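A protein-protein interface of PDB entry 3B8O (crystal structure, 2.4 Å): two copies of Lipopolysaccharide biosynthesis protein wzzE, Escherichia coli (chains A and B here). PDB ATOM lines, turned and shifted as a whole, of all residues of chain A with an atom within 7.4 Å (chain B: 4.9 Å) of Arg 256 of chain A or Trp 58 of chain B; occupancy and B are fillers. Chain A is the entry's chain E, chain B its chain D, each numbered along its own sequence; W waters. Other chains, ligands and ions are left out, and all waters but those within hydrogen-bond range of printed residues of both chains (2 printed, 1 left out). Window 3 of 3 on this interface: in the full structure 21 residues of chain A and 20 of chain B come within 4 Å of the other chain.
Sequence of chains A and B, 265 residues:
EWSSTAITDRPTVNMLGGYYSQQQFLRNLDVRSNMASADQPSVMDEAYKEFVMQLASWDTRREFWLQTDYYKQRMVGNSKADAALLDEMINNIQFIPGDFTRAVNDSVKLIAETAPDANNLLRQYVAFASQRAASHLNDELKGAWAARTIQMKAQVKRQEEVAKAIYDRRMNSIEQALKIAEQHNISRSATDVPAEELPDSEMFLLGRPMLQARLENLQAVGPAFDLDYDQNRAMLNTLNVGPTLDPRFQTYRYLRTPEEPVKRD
No position is printed for both chains.
OG of Ser 57 of chain B sits at hydrogen-bond distance from O of Leu 255 of chain A (2.7 Å).
The backbone carbonyl oxygen (O) of Leu 255 of chain A lies within hydrogen-bond range of the backbone NH (N) of Trp 58 of chain B, at 3.4 Å.
N of Asp 59 of chain B lies within hydrogen-bond range of O of Leu 255 of chain A, at 3.3 Å.
The side-chain carboxylate (OD2) of Asp 59 of chain B is in hydrogen-bond range of the side-chain hydroxyl (OG1) of Thr 257 of chain A (2.6 Å).
OE1 of Glu 259 of chain A is in salt-bridge range of NH2 of Arg 62 of chain B (3.1 Å).
Of chain A, only Leu 255 and Arg 256 come within 4 Å of Trp 58 of chain B.
Of the printed residues of chain B, Leu 255 of chain A touches Ser 57 (2.7 Å), Trp 58 (3.4 Å) and Asp 59 (3.3 Å).
Of the printed residues of chain A, Arg 62 of chain B touches Glu 259 (3.1 Å).
Of the printed residues of chain B, Glu 259 of chain A touches Arg 62 (3.1 Å).
Of the printed residues of chain A, Ser 57 of chain B touches Leu 255.
Printed residues of chain B within 4 Å of Thr 257 of chain A: Asp 59.
Pro 261 of chain A touches none of the printed residues of chain B.
Pro 258 of chain A touches none of the printed residues of chain B.
The nearest printed residue of chain B that does not touch Tyr 254 of chain A is Ser 57 of chain B (5.3 Å).
Of the 20 printed residues of chain A, 5 touch a printed residue of chain B.
Hydrophobic or aromatic side chains of chain B within 4 Å of the printed part of chain A: Trp 58.
Among the printed residues, 8 pairs touch across the chains.
Among the printed residues, Asp or Glu carboxylates within 4 Å of a Lys or Arg side-chain nitrogen of the other chain: Glu 259 of chain A with Arg 62 of chain B.
OG of Ser 57 of chain B is in hydrogen-bond range of N of Asp 59 of chain B.
The backbone NH (N) of Thr 60 of chain B is in hydrogen-bond range of the side-chain hydroxyl (OG) of Ser 57 of chain B (3.1 Å).
NE of Arg 61 of chain B sits at hydrogen-bond distance from O of Ser 57 of chain B, 3.2 Å away.
The side-chain hydroxyl (OG) of Ser 4 of chain A is in hydrogen-bond range of the backbone carbonyl oxygen (O) of Glu 259 of chain A (2.7 Å).
O of Ile 7 of chain A is in hydrogen-bond range of N of Leu 255 of chain A (2.7 Å).
N of Ile 7 of chain A sits at hydrogen-bond distance from O of Arg 256 of chain A, 3.0 Å away.
Tyr 254 of chain A touches Asp 59 of chain B (CB to OD2, 3.9998 Å).
Arg 256 of chain A touches Trp 58 of chain B.
Asp 59 of chain B touches Arg 256 of chain A (OD1 to CA, 3.5 Å).
Water W1 bridges OD2 of Asp 59 of chain B (2.6 Å) and O of Tyr 254 of chain A (3.0 Å).
Water W2 bridges N of Trp 58 of chain B (2.8 Å) and O of Leu 255 of chain A (3.2 Å).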
ATOM      1  N   SER A   3     -37.083   8.063  -7.022  1.00  0.00           N
ATOM      2  CA  SER A   3     -36.060   8.688  -6.189  1.00  0.00           C
ATOM      3  C   SER A   3     -34.851   9.190  -6.991  1.00  0.00           C
ATOM      4  O   SER A   3     -34.569   8.712  -8.072  1.00  0.00           O
ATOM      5  CB  SER A   3     -35.634   7.751  -5.063  1.00  0.00           C
ATOM      6  OG  SER A   3     -35.200   6.537  -5.596  1.00  0.00           O
ATOM      7  N   SER A   4     -34.180  10.194  -6.474  1.00  0.00           N
ATOM      8  CA  SER A   4     -32.932  10.622  -7.018  1.00  0.00           C
ATOM      9  C   SER A   4     -31.894  10.289  -6.006  1.00  0.00           C
ATOM     10  O   SER A   4     -32.231  10.054  -4.831  1.00  0.00           O
ATOM     11  CB  SER A   4     -32.921  12.129  -7.213  1.00  0.00           C
ATOM     12  OG  SER A   4     -33.409  12.446  -8.494  1.00  0.00           O
ATOM     13  N   THR A   5     -30.639  10.309  -6.454  1.00  0.00           N
ATOM     14  CA  THR A   5     -29.492  10.011  -5.630  1.00  0.00           C
ATOM     15  C   THR A   5     -28.441  11.074  -5.881  1.00  0.00           C
ATOM     16  O   THR A   5     -28.280  11.566  -7.011  1.00  0.00           O
ATOM     17  CB  THR A   5     -28.904   8.660  -6.037  1.00  0.00           C
ATOM     18  OG1 THR A   5     -29.904   7.669  -5.833  1.00  0.00           O
ATOM     19  CG2 THR A   5     -27.652   8.290  -5.191  1.00  0.00           C
ATOM     20  N   ALA A   6     -27.743  11.467  -4.821  1.00  0.00           N
ATOM     21  CA  ALA A   6     -26.573  12.315  -4.979  1.00  0.00           C
ATOM     22  C   ALA A   6     -25.436  11.699  -4.180  1.00  0.00           C
ATOM     23  O   ALA A   6     -25.666  11.081  -3.125  1.00  0.00           O
ATOM     24  CB  ALA A   6     -26.855  13.720  -4.559  1.00  0.00           C
ATOM     25  N   ILE A   7     -24.227  11.827  -4.720  1.00  0.00           N
ATOM     26  CA  ILE A   7     -23.015  11.381  -4.024  1.00  0.00           C
ATOM     27  C   ILE A   7     -22.125  12.629  -3.887  1.00  0.00           C
ATOM     28  O   ILE A   7     -21.972  13.383  -4.857  1.00  0.00           O
ATOM     29  CB  ILE A   7     -22.317  10.240  -4.770  1.00  0.00           C
ATOM     30  CG1 ILE A   7     -23.247   9.033  -4.855  1.00  0.00           C
ATOM     31  CG2 ILE A   7     -21.018   9.811  -4.077  1.00  0.00           C
ATOM     32  CD1 ILE A   7     -22.723   7.889  -5.707  1.00  0.00           C
ATOM     33  N   THR A   8     -21.580  12.875  -2.694  1.00  0.00           N
ATOM     34  CA  THR A   8     -20.846  14.109  -2.466  1.00  0.00           C
ATOM     35  C   THR A   8     -19.474  13.831  -1.883  1.00  0.00           C
ATOM     36  O   THR A   8     -19.194  12.737  -1.368  1.00  0.00           O
ATOM     37  CB  THR A   8     -21.608  15.059  -1.493  1.00  0.00           C
ATOM     38  OG1 THR A   8     -21.692  14.430  -0.197  1.00  0.00           O
ATOM     39  CG2 THR A   8     -23.073  15.458  -2.029  1.00  0.00           C
ATOM     40  N   ASP A   9     -18.613  14.838  -1.956  1.00  0.00           N
ATOM     41  CA  ASP A   9     -17.360  14.855  -1.198  1.00  0.00           C
ATOM     42  C   ASP A   9     -16.988  16.318  -0.910  1.00  0.00           C
ATOM     43  O   ASP A   9     -17.598  17.261  -1.452  1.00  0.00           O
ATOM     44  CB  ASP A   9     -16.222  14.117  -1.943  1.00  0.00           C
ATOM     45  CG  ASP A   9     -15.131  13.587  -1.009  1.00  0.00           C
ATOM     46  OD1 ASP A   9     -15.284  13.626   0.228  1.00  0.00           O
ATOM     47  OD2 ASP A   9     -14.093  13.108  -1.510  1.00  0.00           O
ATOM     48  N   SER A 107     -23.897   9.487   0.450  1.00  0.00           N
ATOM     49  CA  SER A 107     -24.946   9.594  -0.543  1.00  0.00           C
ATOM     50  C   SER A 107     -26.253   9.849   0.170  1.00  0.00           C
ATOM     51  O   SER A 107     -26.451   9.409   1.306  1.00  0.00           O
ATOM     52  CB  SER A 107     -25.037   8.344  -1.438  1.00  0.00           C
ATOM     53  OG  SER A 107     -25.343   7.194  -0.698  1.00  0.00           O
ATOM     54  N   VAL A 108     -27.119  10.593  -0.509  1.00  0.00           N
ATOM     55  CA  VAL A 108     -28.407  10.975  -0.005  1.00  0.00           C
ATOM     56  C   VAL A 108     -29.408  10.601  -1.110  1.00  0.00           C
ATOM     57  O   VAL A 108     -29.144  10.805  -2.291  1.00  0.00           O
ATOM     58  CB  VAL A 108     -28.409  12.481   0.256  1.00  0.00           C
ATOM     59  CG1 VAL A 108     -28.073  13.248  -1.035  1.00  0.00           C
ATOM     60  CG2 VAL A 108     -29.711  12.941   0.937  1.00  0.00           C
ATOM     61  N   LEU A 122     -34.275  16.930  -4.885  1.00  0.00           N
ATOM     62  CA  LEU A 122     -32.925  16.565  -4.429  1.00  0.00           C
ATOM     63  C   LEU A 122     -31.911  17.697  -4.727  1.00  0.00           C
ATOM     64  O   LEU A 122     -31.139  18.026  -3.846  1.00  0.00           O
ATOM     65  CB  LEU A 122     -32.423  15.211  -4.964  1.00  0.00           C
ATOM     66  CG  LEU A 122     -31.177  14.729  -4.180  1.00  0.00           C
ATOM     67  CD1 LEU A 122     -31.363  14.834  -2.626  1.00  0.00           C
ATOM     68  CD2 LEU A 122     -30.822  13.302  -4.513  1.00  0.00           C
ATOM     69  N   VAL A 126     -29.964  19.689  -1.578  1.00  0.00           N
ATOM     70  CA  VAL A 126     -28.525  19.719  -1.413  1.00  0.00           C
ATOM     71  C   VAL A 126     -28.072  21.180  -1.336  1.00  0.00           C
ATOM     72  O   VAL A 126     -27.271  21.531  -0.480  1.00  0.00           O
ATOM     73  CB  VAL A 126     -27.835  18.861  -2.507  1.00  0.00           C
ATOM     74  CG1 VAL A 126     -26.367  19.198  -2.680  1.00  0.00           C
ATOM     75  CG2 VAL A 126     -27.965  17.429  -2.142  1.00  0.00           C
ATOM     76  N   ARG A 253     -18.627  18.984  -2.990  1.00  0.00           N
ATOM     77  CA  ARG A 253     -18.787  18.801  -4.421  1.00  0.00           C
ATOM     78  C   ARG A 253     -19.546  17.530  -4.736  1.00  0.00           C
ATOM     79  O   ARG A 253     -19.632  16.636  -3.907  1.00  0.00           O
ATOM     80  CB  ARG A 253     -17.485  18.916  -5.221  1.00  0.00           C
ATOM     81  CG  ARG A 253     -16.478  17.818  -5.063  1.00  0.00           C
ATOM     82  CD  ARG A 253     -15.652  17.753  -6.333  1.00  0.00           C
ATOM     83  NE  ARG A 253     -14.316  17.280  -6.048  1.00  0.00           N
ATOM     84  CZ  ARG A 253     -13.354  17.046  -6.935  1.00  0.00           C
ATOM     85  NH1 ARG A 253     -13.520  17.226  -8.226  1.00  0.00           N
ATOM     86  NH2 ARG A 253     -12.192  16.632  -6.500  1.00  0.00           N
ATOM     87  N   TYR A 254     -20.104  17.484  -5.943  1.00  0.00           N
ATOM     88  CA  TYR A 254     -20.829  16.329  -6.463  1.00  0.00           C
ATOM     89  C   TYR A 254     -19.929  15.290  -7.088  1.00  0.00           C
ATOM     90  O   TYR A 254     -19.135  15.626  -7.945  1.00  0.00           O
ATOM     91  CB  TYR A 254     -21.788  16.821  -7.540  1.00  0.00           C
ATOM     92  CG  TYR A 254     -23.124  17.342  -7.033  1.00  0.00           C
ATOM     93  CD1 TYR A 254     -23.870  16.597  -6.147  1.00  0.00           C
ATOM     94  CD2 TYR A 254     -23.670  18.535  -7.516  1.00  0.00           C
ATOM     95  CE1 TYR A 254     -25.127  17.034  -5.697  1.00  0.00           C
ATOM     96  CE2 TYR A 254     -24.943  19.001  -7.068  1.00  0.00           C
ATOM     97  CZ  TYR A 254     -25.654  18.237  -6.148  1.00  0.00           C
ATOM     98  OH  TYR A 254     -26.907  18.624  -5.670  1.00  0.00           O
ATOM     99  N   LEU A 255     -20.059  14.027  -6.698  1.00  0.00           N
ATOM    100  CA  LEU A 255     -19.494  12.934  -7.513  1.00  0.00           C
ATOM    101  C   LEU A 255     -20.613  12.369  -8.397  1.00  0.00           C
ATOM    102  O   LEU A 255     -20.356  11.714  -9.422  1.00  0.00           O
ATOM    103  CB  LEU A 255     -18.929  11.819  -6.643  1.00  0.00           C
ATOM    104  CG  LEU A 255     -17.888  12.213  -5.596  1.00  0.00           C
ATOM    105  CD1 LEU A 255     -17.325  10.978  -4.879  1.00  0.00           C
ATOM    106  CD2 LEU A 255     -16.783  13.029  -6.251  1.00  0.00           C
ATOM    107  N   ARG A 256     -21.855  12.613  -7.953  1.00  0.00           N
ATOM    108  CA  ARG A 256     -23.052  12.209  -8.661  1.00  0.00           C
ATOM    109  C   ARG A 256     -24.141  13.213  -8.381  1.00  0.00           C
ATOM    110  O   ARG A 256     -24.585  13.398  -7.249  1.00  0.00           O
ATOM    111  CB  ARG A 256     -23.529  10.834  -8.220  1.00  0.00           C
ATOM    112  CG  ARG A 256     -24.871  10.459  -8.789  1.00  0.00           C
ATOM    113  CD  ARG A 256     -25.098   8.998  -8.733  1.00  0.00           C
ATOM    114  NE  ARG A 256     -26.319   8.680  -9.451  1.00  0.00           N
ATOM    115  CZ  ARG A 256     -26.928   7.490  -9.433  1.00  0.00           C
ATOM    116  NH1 ARG A 256     -26.419   6.470  -8.752  1.00  0.00           N
ATOM    117  NH2 ARG A 256     -28.061   7.309 -10.118  1.00  0.00           N
ATOM    118  N   THR A 257     -24.532  13.879  -9.453  1.00  0.00           N
ATOM    119  CA  THR A 257     -25.488  14.937  -9.416  1.00  0.00           C
ATOM    120  C   THR A 257     -26.803  14.209  -9.542  1.00  0.00           C
ATOM    121  O   THR A 257     -26.887  13.208 -10.274  1.00  0.00           O
ATOM    122  CB  THR A 257     -25.207  15.902 -10.606  1.00  0.00           C
ATOM    123  OG1 THR A 257     -23.856  16.382 -10.497  1.00  0.00           O
ATOM    124  CG2 THR A 257     -26.170  17.128 -10.624  1.00  0.00           C
ATOM    125  N   PRO A 258     -27.835  14.679  -8.813  1.00  0.00           N
ATOM    126  CA  PRO A 258     -29.156  14.098  -8.951  1.00  0.00           C
ATOM    127  C   PRO A 258     -29.574  14.236 -10.397  1.00  0.00           C
ATOM    128  O   PRO A 258     -29.261  15.262 -11.012  1.00  0.00           O
ATOM    129  CB  PRO A 258     -30.027  15.020  -8.103  1.00  0.00           C
ATOM    130  CG  PRO A 258     -29.075  15.616  -7.111  1.00  0.00           C
ATOM    131  CD  PRO A 258     -27.814  15.790  -7.840  1.00  0.00           C
ATOM    132  N   GLU A 259     -30.221  13.198 -10.921  1.00  0.00           N
ATOM    133  CA  GLU A 259     -30.865  13.186 -12.227  1.00  0.00           C
ATOM    134  C   GLU A 259     -32.313  12.624 -12.115  1.00  0.00           C
ATOM    135  O   GLU A 259     -32.709  12.119 -11.069  1.00  0.00           O
ATOM    136  CB  GLU A 259     -30.036  12.357 -13.234  1.00  0.00           C
ATOM    137  CG  GLU A 259     -28.603  12.876 -13.513  1.00  0.00           C
ATOM    138  CD  GLU A 259     -28.516  14.207 -14.311  1.00  0.00           C
ATOM    139  OE1 GLU A 259     -29.422  14.507 -15.119  1.00  0.00           O
ATOM    140  OE2 GLU A 259     -27.506  14.945 -14.161  1.00  0.00           O
ATOM    141  N   GLU A 260     -33.099  12.743 -13.183  1.00  0.00           N
ATOM    142  CA  GLU A 260     -34.414  12.122 -13.266  1.00  0.00           C
ATOM    143  C   GLU A 260     -34.290  10.624 -13.244  1.00  0.00           C
ATOM    144  O   GLU A 260     -33.605  10.064 -14.064  1.00  0.00           O
ATOM    145  CB  GLU A 260     -35.184  12.532 -14.521  1.00  0.00           C
ATOM    146  CG  GLU A 260     -36.164  13.648 -14.293  1.00  0.00           C
ATOM    147  CD  GLU A 260     -37.173  13.846 -15.440  1.00  0.00           C
ATOM    148  OE1 GLU A 260     -37.544  12.854 -16.134  1.00  0.00           O
ATOM    149  OE2 GLU A 260     -37.604  15.013 -15.636  1.00  0.00           O
ATOM    150  N   PRO A 261     -34.947   9.974 -12.279  1.00  0.00           N
ATOM    151  CA  PRO A 261     -34.930   8.512 -12.307  1.00  0.00           C
ATOM    152  C   PRO A 261     -35.609   7.987 -13.582  1.00  0.00           C
ATOM    153  O   PRO A 261     -36.537   8.620 -14.120  1.00  0.00           O
ATOM    154  CB  PRO A 261     -35.711   8.111 -11.056  1.00  0.00           C
ATOM    155  CG  PRO A 261     -36.455   9.366 -10.640  1.00  0.00           C
ATOM    156  CD  PRO A 261     -35.717  10.528 -11.150  1.00  0.00           C
ATOM    157  N   ALA B  56     -14.207   7.112 -11.379  1.00  0.00           N
ATOM    158  CA  ALA B  56     -15.293   6.374 -10.749  1.00  0.00           C
ATOM    159  C   ALA B  56     -16.610   7.160 -10.703  1.00  0.00           C
ATOM    160  O   ALA B  56     -17.664   6.589 -10.416  1.00  0.00           O
ATOM    161  CB  ALA B  56     -14.906   5.951  -9.312  1.00  0.00           C
ATOM    162  N   SER B  57     -16.547   8.459 -10.930  1.00  0.00           N
ATOM    163  CA  SER B  57     -17.734   9.314 -10.807  1.00  0.00           C
ATOM    164  C   SER B  57     -18.858   8.960 -11.810  1.00  0.00           C
ATOM    165  O   SER B  57     -18.622   8.708 -12.992  1.00  0.00           O
ATOM    166  CB  SER B  57     -17.327  10.777 -10.939  1.00  0.00           C
ATOM    167  OG  SER B  57     -18.421  11.598 -11.283  1.00  0.00           O
ATOM    168  N   TRP B  58     -20.068   8.898 -11.292  1.00  0.00           N
ATOM    169  CA  TRP B  58     -21.277   8.791 -12.097  1.00  0.00           C
ATOM    170  C   TRP B  58     -21.377   9.958 -13.085  1.00  0.00           C
ATOM    171  O   TRP B  58     -21.639   9.735 -14.268  1.00  0.00           O
ATOM    172  CB  TRP B  58     -22.498   8.778 -11.168  1.00  0.00           C
ATOM    173  CG  TRP B  58     -23.812   8.565 -11.847  1.00  0.00           C
ATOM    174  CD1 TRP B  58     -24.597   9.517 -12.465  1.00  0.00           C
ATOM    175  CD2 TRP B  58     -24.524   7.327 -11.945  1.00  0.00           C
ATOM    176  NE1 TRP B  58     -25.748   8.924 -12.951  1.00  0.00           N
ATOM    177  CE2 TRP B  58     -25.732   7.590 -12.641  1.00  0.00           C
ATOM    178  CE3 TRP B  58     -24.259   6.026 -11.507  1.00  0.00           C
ATOM    179  CZ2 TRP B  58     -26.677   6.602 -12.919  1.00  0.00           C
ATOM    180  CZ3 TRP B  58     -25.213   5.008 -11.783  1.00  0.00           C
ATOM    181  CH2 TRP B  58     -26.414   5.312 -12.491  1.00  0.00           C
ATOM    182  N   ASP B  59     -21.163  11.188 -12.599  1.00  0.00           N
ATOM    183  CA  ASP B  59     -21.191  12.342 -13.485  1.00  0.00           C
ATOM    184  C   ASP B  59     -20.211  12.167 -14.629  1.00  0.00           C
ATOM    185  O   ASP B  59     -20.525  12.516 -15.748  1.00  0.00           O
ATOM    186  CB  ASP B  59     -20.862  13.639 -12.801  1.00  0.00           C
ATOM    187  CG  ASP B  59     -21.956  14.125 -11.884  1.00  0.00           C
ATOM    188  OD1 ASP B  59     -23.100  13.593 -11.893  1.00  0.00           O
ATOM    189  OD2 ASP B  59     -21.648  15.063 -11.130  1.00  0.00           O
ATOM    190  N   THR B  60     -19.032  11.613 -14.363  1.00  0.00           N
ATOM    191  CA  THR B  60     -18.044  11.553 -15.414  1.00  0.00           C
ATOM    192  C   THR B  60     -18.447  10.531 -16.478  1.00  0.00           C
ATOM    193  O   THR B  60     -18.258  10.753 -17.677  1.00  0.00           O
ATOM    194  CB  THR B  60     -16.635  11.337 -14.858  1.00  0.00           C
ATOM    195  OG1 THR B  60     -16.298  12.455 -14.058  1.00  0.00           O
ATOM    196  CG2 THR B  60     -15.548  11.180 -16.015  1.00  0.00           C
ATOM    197  N   ARG B  61     -19.034   9.428 -16.048  1.00  0.00           N
ATOM    198  CA  ARG B  61     -19.489   8.413 -16.998  1.00  0.00           C
ATOM    199  C   ARG B  61     -20.651   8.916 -17.859  1.00  0.00           C
ATOM    200  O   ARG B  61     -20.694   8.687 -19.078  1.00  0.00           O
ATOM    201  CB  ARG B  61     -19.838   7.171 -16.251  1.00  0.00           C
ATOM    202  CG  ARG B  61     -18.594   6.421 -15.694  1.00  0.00           C
ATOM    203  CD  ARG B  61     -19.045   5.233 -14.870  1.00  0.00           C
ATOM    204  NE  ARG B  61     -19.321   5.650 -13.508  1.00  0.00           N
ATOM    205  CZ  ARG B  61     -20.099   5.009 -12.650  1.00  0.00           C
ATOM    206  NH1 ARG B  61     -20.773   3.934 -13.031  1.00  0.00           N
ATOM    207  NH2 ARG B  61     -20.214   5.466 -11.412  1.00  0.00           N
ATOM    208  N   ARG B  62     -21.552   9.666 -17.232  1.00  0.00           N
ATOM    209  CA  ARG B  62     -22.703  10.234 -17.904  1.00  0.00           C
ATOM    210  C   ARG B  62     -22.265  11.281 -18.939  1.00  0.00           C
ATOM    211  O   ARG B  62     -22.635  11.185 -20.094  1.00  0.00           O
ATOM    212  CB  ARG B  62     -23.622  10.862 -16.857  1.00  0.00           C
ATOM    213  CG  ARG B  62     -24.820  11.550 -17.419  1.00  0.00           C
ATOM    214  CD  ARG B  62     -25.632  12.182 -16.338  1.00  0.00           C
ATOM    215  NE  ARG B  62     -27.002  12.242 -16.805  1.00  0.00           N
ATOM    216  CZ  ARG B  62     -27.529  13.256 -17.476  1.00  0.00           C
ATOM    217  NH1 ARG B  62     -26.811  14.362 -17.726  1.00  0.00           N
ATOM    218  NH2 ARG B  62     -28.786  13.169 -17.865  1.00  0.00           N
ATOM    219  N   ASP B  87     -28.405   5.268 -18.860  1.00  0.00           N
ATOM    220  CA  ASP B  87     -28.208   4.636 -17.567  1.00  0.00           C
ATOM    221  C   ASP B  87     -27.556   3.255 -17.638  1.00  0.00           C
ATOM    222  O   ASP B  87     -26.707   2.921 -16.828  1.00  0.00           O
ATOM    223  CB  ASP B  87     -29.534   4.551 -16.840  1.00  0.00           C
ATOM    224  CG  ASP B  87     -29.359   4.247 -15.383  1.00  0.00           C
ATOM    225  OD1 ASP B  87     -29.066   5.173 -14.584  1.00  0.00           O
ATOM    226  OD2 ASP B  87     -29.513   3.058 -15.044  1.00  0.00           O
ATOM    227  N   ILE B  90     -23.765   4.019 -18.397  1.00  0.00           N
ATOM    228  CA  ILE B  90     -23.032   4.408 -17.201  1.00  0.00           C
ATOM    229  C   ILE B  90     -22.695   3.152 -16.373  1.00  0.00           C
ATOM    230  O   ILE B  90     -21.555   2.985 -15.917  1.00  0.00           O
ATOM    231  CB  ILE B  90     -23.811   5.479 -16.375  1.00  0.00           C
ATOM    232  CG1 ILE B  90     -23.969   6.764 -17.185  1.00  0.00           C
ATOM    233  CG2 ILE B  90     -23.136   5.778 -15.063  1.00  0.00           C
ATOM    234  CD1 ILE B  90     -25.103   7.657 -16.699  1.00  0.00           C
ATOM    235  N   ASN B  91     -23.676   2.259 -16.234  1.00  0.00           N
ATOM    236  CA  ASN B  91     -23.484   1.007 -15.524  1.00  0.00           C
ATOM    237  C   ASN B  91     -22.555   0.034 -16.233  1.00  0.00           C
ATOM    238  O   ASN B  91     -22.129  -0.919 -15.630  1.00  0.00           O
ATOM    239  CB  ASN B  91     -24.812   0.366 -15.169  1.00  0.00           C
ATOM    240  CG  ASN B  91     -25.539   1.135 -14.061  1.00  0.00           C
ATOM    241  OD1 ASN B  91     -24.935   1.476 -13.038  1.00  0.00           O
ATOM    242  ND2 ASN B  91     -26.826   1.436 -14.270  1.00  0.00           N
HETATM  243  O   HOH W   1     -19.413  16.276 -10.810  1.00  0.00           O
HETATM  244  O   HOH W   2     -20.303   8.687  -8.471  1.00  0.00           O
